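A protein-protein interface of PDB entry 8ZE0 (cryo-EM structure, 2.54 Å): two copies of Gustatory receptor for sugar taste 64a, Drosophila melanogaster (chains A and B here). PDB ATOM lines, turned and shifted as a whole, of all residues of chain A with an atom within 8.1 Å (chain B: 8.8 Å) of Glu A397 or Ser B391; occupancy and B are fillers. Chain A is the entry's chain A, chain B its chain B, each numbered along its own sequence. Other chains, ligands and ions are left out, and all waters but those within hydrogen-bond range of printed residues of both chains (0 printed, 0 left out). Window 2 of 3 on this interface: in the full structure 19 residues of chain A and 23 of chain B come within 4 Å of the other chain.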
ATOM      1  N   CYS A 294       1.721  21.859  20.355  1.00  0.00           N
ATOM      2  CA  CYS A 294       1.415  21.115  21.566  1.00  0.00           C
ATOM      3  C   CYS A 294       1.422  19.612  21.287  1.00  0.00           C
ATOM      4  O   CYS A 294       1.467  19.163  20.139  1.00  0.00           O
ATOM      5  CB  CYS A 294       0.063  21.547  22.133  1.00  0.00           C
ATOM      6  SG  CYS A 294      -0.769  20.290  23.135  1.00  0.00           S
ATOM      7  N   GLU A 295       1.379  18.827  22.366  1.00  0.00           N
ATOM      8  CA  GLU A 295       1.395  17.374  22.227  1.00  0.00           C
ATOM      9  C   GLU A 295       0.103  16.843  21.618  1.00  0.00           C
ATOM     10  O   GLU A 295       0.118  15.797  20.959  1.00  0.00           O
ATOM     11  CB  GLU A 295       1.649  16.715  23.582  1.00  0.00           C
ATOM     12  CG  GLU A 295       2.291  15.341  23.491  1.00  0.00           C
ATOM     13  CD  GLU A 295       2.666  14.778  24.847  1.00  0.00           C
ATOM     14  OE1 GLU A 295       1.877  14.943  25.800  1.00  0.00           O
ATOM     15  OE2 GLU A 295       3.751  14.171  24.960  1.00  0.00           O
ATOM     16  N   SER A 296      -1.019  17.535  21.832  1.00  0.00           N
ATOM     17  CA  SER A 296      -2.295  17.064  21.299  1.00  0.00           C
ATOM     18  C   SER A 296      -2.305  17.084  19.775  1.00  0.00           C
ATOM     19  O   SER A 296      -2.835  16.164  19.138  1.00  0.00           O
ATOM     20  CB  SER A 296      -3.440  17.912  21.854  1.00  0.00           C
ATOM     21  OG  SER A 296      -3.183  18.302  23.191  1.00  0.00           O
ATOM     22  N   VAL A 297      -1.734  18.130  19.171  1.00  0.00           N
ATOM     23  CA  VAL A 297      -1.685  18.212  17.714  1.00  0.00           C
ATOM     24  C   VAL A 297      -0.853  17.070  17.145  1.00  0.00           C
ATOM     25  O   VAL A 297      -1.228  16.445  16.145  1.00  0.00           O
ATOM     26  CB  VAL A 297      -1.144  19.584  17.275  1.00  0.00           C
ATOM     27  CG1 VAL A 297      -1.035  19.656  15.760  1.00  0.00           C
ATOM     28  CG2 VAL A 297      -2.032  20.698  17.808  1.00  0.00           C
ATOM     29  N   PHE A 298       0.288  16.779  17.773  1.00  0.00           N
ATOM     30  CA  PHE A 298       1.121  15.673  17.316  1.00  0.00           C
ATOM     31  C   PHE A 298       0.421  14.335  17.515  1.00  0.00           C
ATOM     32  O   PHE A 298       0.559  13.429  16.685  1.00  0.00           O
ATOM     33  CB  PHE A 298       2.465  15.695  18.039  1.00  0.00           C
ATOM     34  CG  PHE A 298       3.433  16.696  17.481  1.00  0.00           C
ATOM     35  CD1 PHE A 298       3.761  16.681  16.136  1.00  0.00           C
ATOM     36  CD2 PHE A 298       4.011  17.653  18.298  1.00  0.00           C
ATOM     37  CE1 PHE A 298       4.650  17.601  15.616  1.00  0.00           C
ATOM     38  CE2 PHE A 298       4.904  18.573  17.783  1.00  0.00           C
ATOM     39  CZ  PHE A 298       5.222  18.547  16.440  1.00  0.00           C
ATOM     40  N   ILE A 299      -0.337  14.193  18.604  1.00  0.00           N
ATOM     41  CA  ILE A 299      -1.117  12.975  18.817  1.00  0.00           C
ATOM     42  C   ILE A 299      -2.125  12.794  17.691  1.00  0.00           C
ATOM     43  O   ILE A 299      -2.278  11.699  17.137  1.00  0.00           O
ATOM     44  CB  ILE A 299      -1.813  13.016  20.190  1.00  0.00           C
ATOM     45  CG1 ILE A 299      -0.818  12.723  21.312  1.00  0.00           C
ATOM     46  CG2 ILE A 299      -2.967  12.026  20.238  1.00  0.00           C
ATOM     47  CD1 ILE A 299      -1.300  13.154  22.681  1.00  0.00           C
ATOM     48  N   GLN A 300      -2.824  13.874  17.334  1.00  0.00           N
ATOM     49  CA  GLN A 300      -3.811  13.800  16.262  1.00  0.00           C
ATOM     50  C   GLN A 300      -3.158  13.461  14.927  1.00  0.00           C
ATOM     51  O   GLN A 300      -3.677  12.638  14.162  1.00  0.00           O
ATOM     52  CB  GLN A 300      -4.579  15.118  16.167  1.00  0.00           C
ATOM     53  CG  GLN A 300      -5.822  15.043  15.301  1.00  0.00           C
ATOM     54  CD  GLN A 300      -6.758  16.213  15.524  1.00  0.00           C
ATOM     55  OE1 GLN A 300      -6.604  16.973  16.479  1.00  0.00           O
ATOM     56  NE2 GLN A 300      -7.737  16.362  14.639  1.00  0.00           N
ATOM     57  N   ILE A 301      -2.015  14.086  14.633  1.00  0.00           N
ATOM     58  CA  ILE A 301      -1.319  13.819  13.376  1.00  0.00           C
ATOM     59  C   ILE A 301      -0.858  12.369  13.318  1.00  0.00           C
ATOM     60  O   ILE A 301      -1.003  11.697  12.290  1.00  0.00           O
ATOM     61  CB  ILE A 301      -0.141  14.794  13.198  1.00  0.00           C
ATOM     62  CG1 ILE A 301      -0.652  16.225  13.032  1.00  0.00           C
ATOM     63  CG2 ILE A 301       0.706  14.397  11.999  1.00  0.00           C
ATOM     64  CD1 ILE A 301       0.428  17.273  13.149  1.00  0.00           C
ATOM     65  N   ARG A 302      -0.298  11.863  14.421  1.00  0.00           N
ATOM     66  CA  ARG A 302       0.164  10.480  14.452  1.00  0.00           C
ATOM     67  C   ARG A 302      -0.998   9.507  14.309  1.00  0.00           C
ATOM     68  O   ARG A 302      -0.884   8.493  13.612  1.00  0.00           O
ATOM     69  CB  ARG A 302       0.935  10.210  15.742  1.00  0.00           C
ATOM     70  CG  ARG A 302       1.789   8.953  15.697  1.00  0.00           C
ATOM     71  CD  ARG A 302       2.293   8.573  17.079  1.00  0.00           C
ATOM     72  NE  ARG A 302       1.232   8.615  18.078  1.00  0.00           N
ATOM     73  CZ  ARG A 302       0.332   7.656  18.256  1.00  0.00           C
ATOM     74  NH1 ARG A 302       0.337   6.558  17.519  1.00  0.00           N
ATOM     75  NH2 ARG A 302      -0.594   7.804  19.198  1.00  0.00           N
ATOM     76  N   GLU A 303      -2.128   9.795  14.960  1.00  0.00           N
ATOM     77  CA  GLU A 303      -3.289   8.919  14.845  1.00  0.00           C
ATOM     78  C   GLU A 303      -3.834   8.905  13.422  1.00  0.00           C
ATOM     79  O   GLU A 303      -4.197   7.843  12.902  1.00  0.00           O
ATOM     80  CB  GLU A 303      -4.371   9.350  15.834  1.00  0.00           C
ATOM     81  CG  GLU A 303      -4.090   8.945  17.271  1.00  0.00           C
ATOM     82  CD  GLU A 303      -5.170   9.407  18.228  1.00  0.00           C
ATOM     83  OE1 GLU A 303      -5.930  10.330  17.869  1.00  0.00           O
ATOM     84  OE2 GLU A 303      -5.260   8.847  19.341  1.00  0.00           O
ATOM     85  N   LEU A 386       9.057  17.463  10.016  1.00  0.00           N
ATOM     86  CA  LEU A 386       9.108  17.008  11.401  1.00  0.00           C
ATOM     87  C   LEU A 386      10.522  17.067  11.965  1.00  0.00           C
ATOM     88  O   LEU A 386      10.697  17.267  13.174  1.00  0.00           O
ATOM     89  CB  LEU A 386       8.553  15.589  11.509  1.00  0.00           C
ATOM     90  CG  LEU A 386       7.030  15.479  11.579  1.00  0.00           C
ATOM     91  CD1 LEU A 386       6.605  14.022  11.543  1.00  0.00           C
ATOM     92  CD2 LEU A 386       6.498  16.168  12.827  1.00  0.00           C
ATOM     93  N   SER A 393       9.534  21.763  21.908  1.00  0.00           N
ATOM     94  CA  SER A 393       8.272  21.174  21.483  1.00  0.00           C
ATOM     95  C   SER A 393       8.458  19.767  20.927  1.00  0.00           C
ATOM     96  O   SER A 393       7.670  19.318  20.088  1.00  0.00           O
ATOM     97  CB  SER A 393       7.587  22.070  20.451  1.00  0.00           C
ATOM     98  OG  SER A 393       8.075  21.818  19.147  1.00  0.00           O
ATOM     99  N   TRP A 394       9.493  19.066  21.381  1.00  0.00           N
ATOM    100  CA  TRP A 394       9.771  17.697  20.971  1.00  0.00           C
ATOM    101  C   TRP A 394       9.323  16.763  22.088  1.00  0.00           C
ATOM    102  O   TRP A 394       9.753  16.914  23.236  1.00  0.00           O
ATOM    103  CB  TRP A 394      11.259  17.517  20.673  1.00  0.00           C
ATOM    104  CG  TRP A 394      11.668  16.104  20.392  1.00  0.00           C
ATOM    105  CD1 TRP A 394      12.089  15.177  21.299  1.00  0.00           C
ATOM    106  CD2 TRP A 394      11.720  15.464  19.112  1.00  0.00           C
ATOM    107  NE1 TRP A 394      12.388  13.995  20.666  1.00  0.00           N
ATOM    108  CE2 TRP A 394      12.171  14.147  19.321  1.00  0.00           C
ATOM    109  CE3 TRP A 394      11.423  15.877  17.810  1.00  0.00           C
ATOM    110  CZ2 TRP A 394      12.333  13.240  18.278  1.00  0.00           C
ATOM    111  CZ3 TRP A 394      11.585  14.975  16.777  1.00  0.00           C
ATOM    112  CH2 TRP A 394      12.035  13.672  17.016  1.00  0.00           C
ATOM    113  N   CYS A 395       8.462  15.805  21.754  1.00  0.00           N
ATOM    114  CA  CYS A 395       7.905  14.892  22.742  1.00  0.00           C
ATOM    115  C   CYS A 395       7.964  13.464  22.214  1.00  0.00           C
ATOM    116  O   CYS A 395       8.530  13.195  21.149  1.00  0.00           O
ATOM    117  CB  CYS A 395       6.465  15.280  23.101  1.00  0.00           C
ATOM    118  SG  CYS A 395       5.357  15.438  21.684  1.00  0.00           S
ATOM    119  N   VAL A 396       7.371  12.542  22.973  1.00  0.00           N
ATOM    120  CA  VAL A 396       7.385  11.134  22.591  1.00  0.00           C
ATOM    121  C   VAL A 396       6.582  10.906  21.318  1.00  0.00           C
ATOM    122  O   VAL A 396       6.925  10.036  20.508  1.00  0.00           O
ATOM    123  CB  VAL A 396       6.860  10.265  23.749  1.00  0.00           C
ATOM    124  CG1 VAL A 396       7.262   8.813  23.547  1.00  0.00           C
ATOM    125  CG2 VAL A 396       7.376  10.789  25.081  1.00  0.00           C
ATOM    126  N   GLU A 397       5.502  11.666  21.123  1.00  0.00           N
ATOM    127  CA  GLU A 397       4.675  11.492  19.932  1.00  0.00           C
ATOM    128  C   GLU A 397       5.455  11.806  18.662  1.00  0.00           C
ATOM    129  O   GLU A 397       5.351  11.080  17.664  1.00  0.00           O
ATOM    130  CB  GLU A 397       3.433  12.376  20.031  1.00  0.00           C
ATOM    131  CG  GLU A 397       2.669  12.205  21.330  1.00  0.00           C
ATOM    132  CD  GLU A 397       2.172  10.787  21.530  1.00  0.00           C
ATOM    133  OE1 GLU A 397       1.611  10.213  20.575  1.00  0.00           O
ATOM    134  OE2 GLU A 397       2.345  10.248  22.642  1.00  0.00           O
ATOM    135  N   VAL A 398       6.243  12.884  18.677  1.00  0.00           N
ATOM    136  CA  VAL A 398       7.042  13.233  17.506  1.00  0.00           C
ATOM    137  C   VAL A 398       8.083  12.158  17.236  1.00  0.00           C
ATOM    138  O   VAL A 398       8.351  11.809  16.081  1.00  0.00           O
ATOM    139  CB  VAL A 398       7.696  14.615  17.690  1.00  0.00           C
ATOM    140  CG1 VAL A 398       8.086  15.198  16.342  1.00  0.00           C
ATOM    141  CG2 VAL A 398       6.761  15.549  18.427  1.00  0.00           C
ATOM    142  N   GLU A 399       8.694  11.624  18.296  1.00  0.00           N
ATOM    143  CA  GLU A 399       9.682  10.564  18.127  1.00  0.00           C
ATOM    144  C   GLU A 399       9.048   9.324  17.509  1.00  0.00           C
ATOM    145  O   GLU A 399       9.609   8.719  16.585  1.00  0.00           O
ATOM    146  CB  GLU A 399      10.326  10.237  19.474  1.00  0.00           C
ATOM    147  CG  GLU A 399      11.793   9.858  19.388  1.00  0.00           C
ATOM    148  CD  GLU A 399      12.340   9.345  20.706  1.00  0.00           C
ATOM    149  OE1 GLU A 399      11.756   9.672  21.761  1.00  0.00           O
ATOM    150  OE2 GLU A 399      13.352   8.615  20.688  1.00  0.00           O
ATOM    151  N   ARG A 400       7.867   8.938  17.999  1.00  0.00           N
ATOM    152  CA  ARG A 400       7.165   7.789  17.435  1.00  0.00           C
ATOM    153  C   ARG A 400       6.819   8.020  15.972  1.00  0.00           C
ATOM    154  O   ARG A 400       7.003   7.130  15.135  1.00  0.00           O
ATOM    155  CB  ARG A 400       5.895   7.499  18.234  1.00  0.00           C
ATOM    156  CG  ARG A 400       6.124   7.044  19.661  1.00  0.00           C
ATOM    157  CD  ARG A 400       4.799   6.752  20.348  1.00  0.00           C
ATOM    158  NE  ARG A 400       3.984   5.816  19.581  1.00  0.00           N
ATOM    159  CZ  ARG A 400       2.792   5.375  19.957  1.00  0.00           C
ATOM    160  NH1 ARG A 400       2.237   5.765  21.092  1.00  0.00           N
ATOM    161  NH2 ARG A 400       2.140   4.518  19.176  1.00  0.00           N
ATOM    162  N   LEU A 401       6.312   9.211  15.647  1.00  0.00           N
ATOM    163  CA  LEU A 401       5.922   9.505  14.272  1.00  0.00           C
ATOM    164  C   LEU A 401       7.129   9.486  13.338  1.00  0.00           C
ATOM    165  O   LEU A 401       7.060   8.935  12.231  1.00  0.00           O
ATOM    166  CB  LEU A 401       5.216  10.859  14.221  1.00  0.00           C
ATOM    167  CG  LEU A 401       4.398  11.188  12.974  1.00  0.00           C
ATOM    168  CD1 LEU A 401       3.512  10.013  12.578  1.00  0.00           C
ATOM    169  CD2 LEU A 401       3.576  12.451  13.186  1.00  0.00           C
ATOM    170  N   ILE A 402       8.242  10.086  13.770  1.00  0.00           N
ATOM    171  CA  ILE A 402       9.447  10.112  12.947  1.00  0.00           C
ATOM    172  C   ILE A 402       9.985   8.704  12.743  1.00  0.00           C
ATOM    173  O   ILE A 402      10.368   8.327  11.630  1.00  0.00           O
ATOM    174  CB  ILE A 402      10.503  11.041  13.575  1.00  0.00           C
ATOM    175  CG1 ILE A 402      10.088  12.505  13.410  1.00  0.00           C
ATOM    176  CG2 ILE A 402      11.877  10.788  12.965  1.00  0.00           C
ATOM    177  CD1 ILE A 402      11.229  13.489  13.547  1.00  0.00           C
ATOM    178  N   PHE A 403      10.014   7.899  13.810  1.00  0.00           N
ATOM    179  CA  PHE A 403      10.456   6.515  13.680  1.00  0.00           C
ATOM    180  C   PHE A 403       9.553   5.742  12.727  1.00  0.00           C
ATOM    181  O   PHE A 403      10.035   4.945  11.913  1.00  0.00           O
ATOM    182  CB  PHE A 403      10.482   5.848  15.057  1.00  0.00           C
ATOM    183  CG  PHE A 403      11.170   4.513  15.076  1.00  0.00           C
ATOM    184  CD1 PHE A 403      12.553   4.430  15.075  1.00  0.00           C
ATOM    185  CD2 PHE A 403      10.434   3.341  15.096  1.00  0.00           C
ATOM    186  CE1 PHE A 403      13.188   3.203  15.095  1.00  0.00           C
ATOM    187  CE2 PHE A 403      11.063   2.110  15.113  1.00  0.00           C
ATOM    188  CZ  PHE A 403      12.442   2.043  15.113  1.00  0.00           C
ATOM    189  N   GLN A 404       8.241   5.977  12.804  1.00  0.00           N
ATOM    190  CA  GLN A 404       7.297   5.257  11.956  1.00  0.00           C
ATOM    191  C   GLN A 404       7.497   5.603  10.486  1.00  0.00           C
ATOM    192  O   GLN A 404       7.569   4.708   9.636  1.00  0.00           O
ATOM    193  CB  GLN A 404       5.865   5.562  12.393  1.00  0.00           C
ATOM    194  CG  GLN A 404       4.815   4.701  11.715  1.00  0.00           C
ATOM    195  CD  GLN A 404       3.456   4.817  12.372  1.00  0.00           C
ATOM    196  OE1 GLN A 404       3.328   5.372  13.462  1.00  0.00           O
ATOM    197  NE2 GLN A 404       2.432   4.286  11.713  1.00  0.00           N
ATOM    198  N   GLU B 292      -6.532  -0.931  26.867  1.00  0.00           N
ATOM    199  CA  GLU B 292      -5.385  -0.298  27.502  1.00  0.00           C
ATOM    200  C   GLU B 292      -4.475  -1.363  28.108  1.00  0.00           C
ATOM    201  O   GLU B 292      -4.924  -2.200  28.896  1.00  0.00           O
ATOM    202  CB  GLU B 292      -5.864   0.687  28.570  1.00  0.00           C
ATOM    203  CG  GLU B 292      -6.595   1.948  28.056  1.00  0.00           C
ATOM    204  CD  GLU B 292      -5.845   2.797  27.017  1.00  0.00           C
ATOM    205  OE1 GLU B 292      -4.868   2.342  26.385  1.00  0.00           O
ATOM    206  OE2 GLU B 292      -6.261   3.960  26.829  1.00  0.00           O
ATOM    207  N   LEU B 386       1.326  -2.926  16.930  1.00  0.00           N
ATOM    208  CA  LEU B 386       2.064  -2.197  17.957  1.00  0.00           C
ATOM    209  C   LEU B 386       2.173  -0.712  17.630  1.00  0.00           C
ATOM    210  O   LEU B 386       2.237   0.118  18.543  1.00  0.00           O
ATOM    211  CB  LEU B 386       3.454  -2.804  18.137  1.00  0.00           C
ATOM    212  CG  LEU B 386       3.522  -4.040  19.033  1.00  0.00           C
ATOM    213  CD1 LEU B 386       4.923  -4.624  19.018  1.00  0.00           C
ATOM    214  CD2 LEU B 386       3.093  -3.701  20.452  1.00  0.00           C
ATOM    215  N   ARG B 387       2.198  -0.360  16.342  1.00  0.00           N
ATOM    216  CA  ARG B 387       2.260   1.044  15.954  1.00  0.00           C
ATOM    217  C   ARG B 387       0.983   1.796  16.302  1.00  0.00           C
ATOM    218  O   ARG B 387       0.985   3.031  16.299  1.00  0.00           O
ATOM    219  CB  ARG B 387       2.541   1.164  14.456  1.00  0.00           C
ATOM    220  CG  ARG B 387       3.972   0.844  14.066  1.00  0.00           C
ATOM    221  CD  ARG B 387       4.109   0.678  12.563  1.00  0.00           C
ATOM    222  NE  ARG B 387       5.494   0.457  12.166  1.00  0.00           N
ATOM    223  CZ  ARG B 387       5.874  -0.385  11.215  1.00  0.00           C
ATOM    224  NH1 ARG B 387       4.994  -1.095  10.528  1.00  0.00           N
ATOM    225  NH2 ARG B 387       7.170  -0.521  10.949  1.00  0.00           N
ATOM    226  N   ARG B 388      -0.101   1.083  16.603  1.00  0.00           N
ATOM    227  CA  ARG B 388      -1.378   1.689  16.947  1.00  0.00           C
ATOM    228  C   ARG B 388      -1.612   1.744  18.451  1.00  0.00           C
ATOM    229  O   ARG B 388      -2.734   2.030  18.882  1.00  0.00           O
ATOM    230  CB  ARG B 388      -2.515   0.929  16.264  1.00  0.00           C
ATOM    231  CG  ARG B 388      -2.262   0.668  14.794  1.00  0.00           C
ATOM    232  CD  ARG B 388      -3.277  -0.295  14.215  1.00  0.00           C
ATOM    233  NE  ARG B 388      -2.768  -0.983  13.036  1.00  0.00           N
ATOM    234  CZ  ARG B 388      -3.108  -2.215  12.681  1.00  0.00           C
ATOM    235  NH1 ARG B 388      -3.963  -2.929  13.396  1.00  0.00           N
ATOM    236  NH2 ARG B 388      -2.579  -2.742  11.581  1.00  0.00           N
ATOM    237  N   VAL B 389      -0.583   1.467  19.255  1.00  0.00           N
ATOM    238  CA  VAL B 389      -0.727   1.529  20.704  1.00  0.00           C
ATOM    239  C   VAL B 389      -1.009   2.965  21.127  1.00  0.00           C
ATOM    240  O   VAL B 389      -0.402   3.916  20.618  1.00  0.00           O
ATOM    241  CB  VAL B 389       0.536   0.973  21.384  1.00  0.00           C
ATOM    242  CG1 VAL B 389       0.629   1.436  22.832  1.00  0.00           C
ATOM    243  CG2 VAL B 389       0.555  -0.546  21.304  1.00  0.00           C
ATOM    244  N   SER B 390      -1.949   3.126  22.058  1.00  0.00           N
ATOM    245  CA  SER B 390      -2.353   4.448  22.513  1.00  0.00           C
ATOM    246  C   SER B 390      -1.174   5.195  23.133  1.00  0.00           C
ATOM    247  O   SER B 390      -0.184   4.603  23.572  1.00  0.00           O
ATOM    248  CB  SER B 390      -3.498   4.341  23.520  1.00  0.00           C
ATOM    249  OG  SER B 390      -3.189   3.416  24.547  1.00  0.00           O
ATOM    250  N   SER B 391      -1.293   6.524  23.155  1.00  0.00           N
ATOM    251  CA  SER B 391      -0.177   7.365  23.577  1.00  0.00           C
ATOM    252  C   SER B 391       0.183   7.140  25.040  1.00  0.00           C
ATOM    253  O   SER B 391       1.367   7.012  25.378  1.00  0.00           O
ATOM    254  CB  SER B 391      -0.510   8.837  23.327  1.00  0.00           C
ATOM    255  OG  SER B 391       0.391   9.688  24.014  1.00  0.00           O
ATOM    256  N   ARG B 392      -0.814   7.084  25.927  1.00  0.00           N
ATOM    257  CA  ARG B 392      -0.515   6.989  27.351  1.00  0.00           C
ATOM    258  C   ARG B 392      -0.019   5.606  27.753  1.00  0.00           C
ATOM    259  O   ARG B 392       0.681   5.482  28.763  1.00  0.00           O
ATOM    260  CB  ARG B 392      -1.742   7.343  28.193  1.00  0.00           C
ATOM    261  CG  ARG B 392      -2.840   6.296  28.185  1.00  0.00           C
ATOM    262  CD  ARG B 392      -3.574   6.306  29.516  1.00  0.00           C
ATOM    263  NE  ARG B 392      -3.044   5.307  30.439  1.00  0.00           N
ATOM    264  CZ  ARG B 392      -3.406   4.032  30.466  1.00  0.00           C
ATOM    265  NH1 ARG B 392      -4.310   3.553  29.630  1.00  0.00           N
ATOM    266  NH2 ARG B 392      -2.849   3.218  31.360  1.00  0.00           N
ATOM    267  N   SER B 393      -0.363   4.567  26.988  1.00  0.00           N
ATOM    268  CA  SER B 393       0.081   3.206  27.262  1.00  0.00           C
ATOM    269  C   SER B 393       1.345   2.852  26.487  1.00  0.00           C
ATOM    270  O   SER B 393       1.580   1.678  26.179  1.00  0.00           O
ATOM    271  CB  SER B 393      -1.036   2.211  26.947  1.00  0.00           C
ATOM    272  OG  SER B 393      -1.047   1.867  25.574  1.00  0.00           O
ATOM    273  N   TRP B 394       2.161   3.851  26.167  1.00  0.00           N
ATOM    274  CA  TRP B 394       3.422   3.657  25.465  1.00  0.00           C
ATOM    275  C   TRP B 394       4.553   3.758  26.481  1.00  0.00           C
ATOM    276  O   TRP B 394       4.662   4.761  27.195  1.00  0.00           O
ATOM    277  CB  TRP B 394       3.587   4.698  24.358  1.00  0.00           C
ATOM    278  CG  TRP B 394       4.923   4.677  23.682  1.00  0.00           C
ATOM    279  CD1 TRP B 394       6.035   5.383  24.039  1.00  0.00           C
ATOM    280  CD2 TRP B 394       5.281   3.931  22.514  1.00  0.00           C
ATOM    281  NE1 TRP B 394       7.066   5.113  23.174  1.00  0.00           N
ATOM    282  CE2 TRP B 394       6.628   4.223  22.228  1.00  0.00           C
ATOM    283  CE3 TRP B 394       4.594   3.037  21.687  1.00  0.00           C
ATOM    284  CZ2 TRP B 394       7.302   3.657  21.150  1.00  0.00           C
ATOM    285  CZ3 TRP B 394       5.264   2.477  20.616  1.00  0.00           C
ATOM    286  CH2 TRP B 394       6.604   2.788  20.357  1.00  0.00           C
ATOM    287  N   CYS B 395       5.389   2.725  26.545  1.00  0.00           N
ATOM    288  CA  CYS B 395       6.470   2.668  27.520  1.00  0.00           C
ATOM    289  C   CYS B 395       7.756   2.222  26.836  1.00  0.00           C
ATOM    290  O   CYS B 395       7.815   2.071  25.612  1.00  0.00           O
ATOM    291  CB  CYS B 395       6.116   1.731  28.682  1.00  0.00           C
ATOM    292  SG  CYS B 395       5.626   0.067  28.178  1.00  0.00           S
ATOM    293  N   VAL B 398       7.521  -1.209  24.841  1.00  0.00           N
ATOM    294  CA  VAL B 398       6.960  -1.135  23.495  1.00  0.00           C
ATOM    295  C   VAL B 398       7.991  -0.579  22.523  1.00  0.00           C
ATOM    296  O   VAL B 398       8.098  -1.037  21.381  1.00  0.00           O
ATOM    297  CB  VAL B 398       5.672  -0.293  23.491  1.00  0.00           C
ATOM    298  CG1 VAL B 398       4.834  -0.618  22.265  1.00  0.00           C
ATOM    299  CG2 VAL B 398       4.882  -0.527  24.758  1.00  0.00           C
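The side-chain carboxylate (OE2) of Glu A397 is in hydrogen-bond range of the side-chain hydroxyl (OG) of Ser B391, 2.5 Å away. The guanidinium group (NH2) of Arg A400 lies within hydrogen-bond range of the backbone carbonyl oxygen (O) of Arg B387, 3.4 Å away. NH2 of Arg A400 lies within hydrogen-bond range of O of Val B389 (3.0 Å).
The side-chain carboxylate (OE1) of Glu A397 is in salt-bridge range of the guanidinium group (NE) of Arg A302. The side-chain carboxylate (OE1) of Glu B292 is in hydrogen-bond range of the side-chain hydroxyl (OG) of Ser B390, 2.7 Å away. The side-chain hydroxyl (OG) of Ser B393 sits at hydrogen-bond distance from the side-chain hydroxyl (OG) of Ser B390, at 2.8 Å.
Among the printed residues, merely in contact across the chains: Arg A302 with Arg B387 (3.8 Å), Val A396 with Trp B394 (3.7 Å), Arg A400 with Ser B390 (3.7 Å), Arg A400 with Ser B391 (3.8 Å) and Arg A400 with Trp B394 (3.4 Å).
Printed residues of chain B within 4 Å of Arg A302: Arg B387 (3.8 Å). Of chain B, only Ser B391 (2.5 Å) comes within 4 Å of Glu A397. Of the printed residues of chain B, Arg A400 touches Arg B387 (3.4 Å), Val B389 (3.0 Å), Ser B390 (3.7 Å), Ser B391 (3.8 Å) and Trp B394 (3.4 Å). Printed residues of chain A within 4 Å of Arg B387: Arg A302 and Arg A400. Of the printed residues of chain A, Val B389 touches Arg A400 (3.0 Å). Ser B390 touches just one residue of chain A: Arg A400 (3.7 Å). Ser B391 touches two residues of chain A. Of the printed residues of chain A, Trp B394 touches Val A396 (3.7 Å) and Arg A400 (3.4 Å). The nearest residue of chain A that does not touch Ser B391 is Ile A299 (4.1 Å).
Of the 12 printed residues of chain B, 5 touch a printed residue of chain A. Printed residues of chain B that touch a printed residue of chain A: Arg B387, Val B389, Ser B390, Ser B391 and Trp B394. Hydrophobic or aromatic side chains of chain B that line the printed part of chain A: Trp B394. Along chain B the printed residues that touch a printed residue of chain A span positions 387 to 394. Of the 23 printed residues of chain A, 4 touch a printed residue of chain B. Hydrophobic or aromatic side chains of chain A that line the printed part of chain B: Val A396. Among the printed residues, 8 pairs touch across the chains. Among the printed residues, no Asp or Glu carboxylate lies within 4 Å of a Lys or Arg side-chain nitrogen of the other chain.
Positions printed for both chains: 386, 393, 394, 395 and 398.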
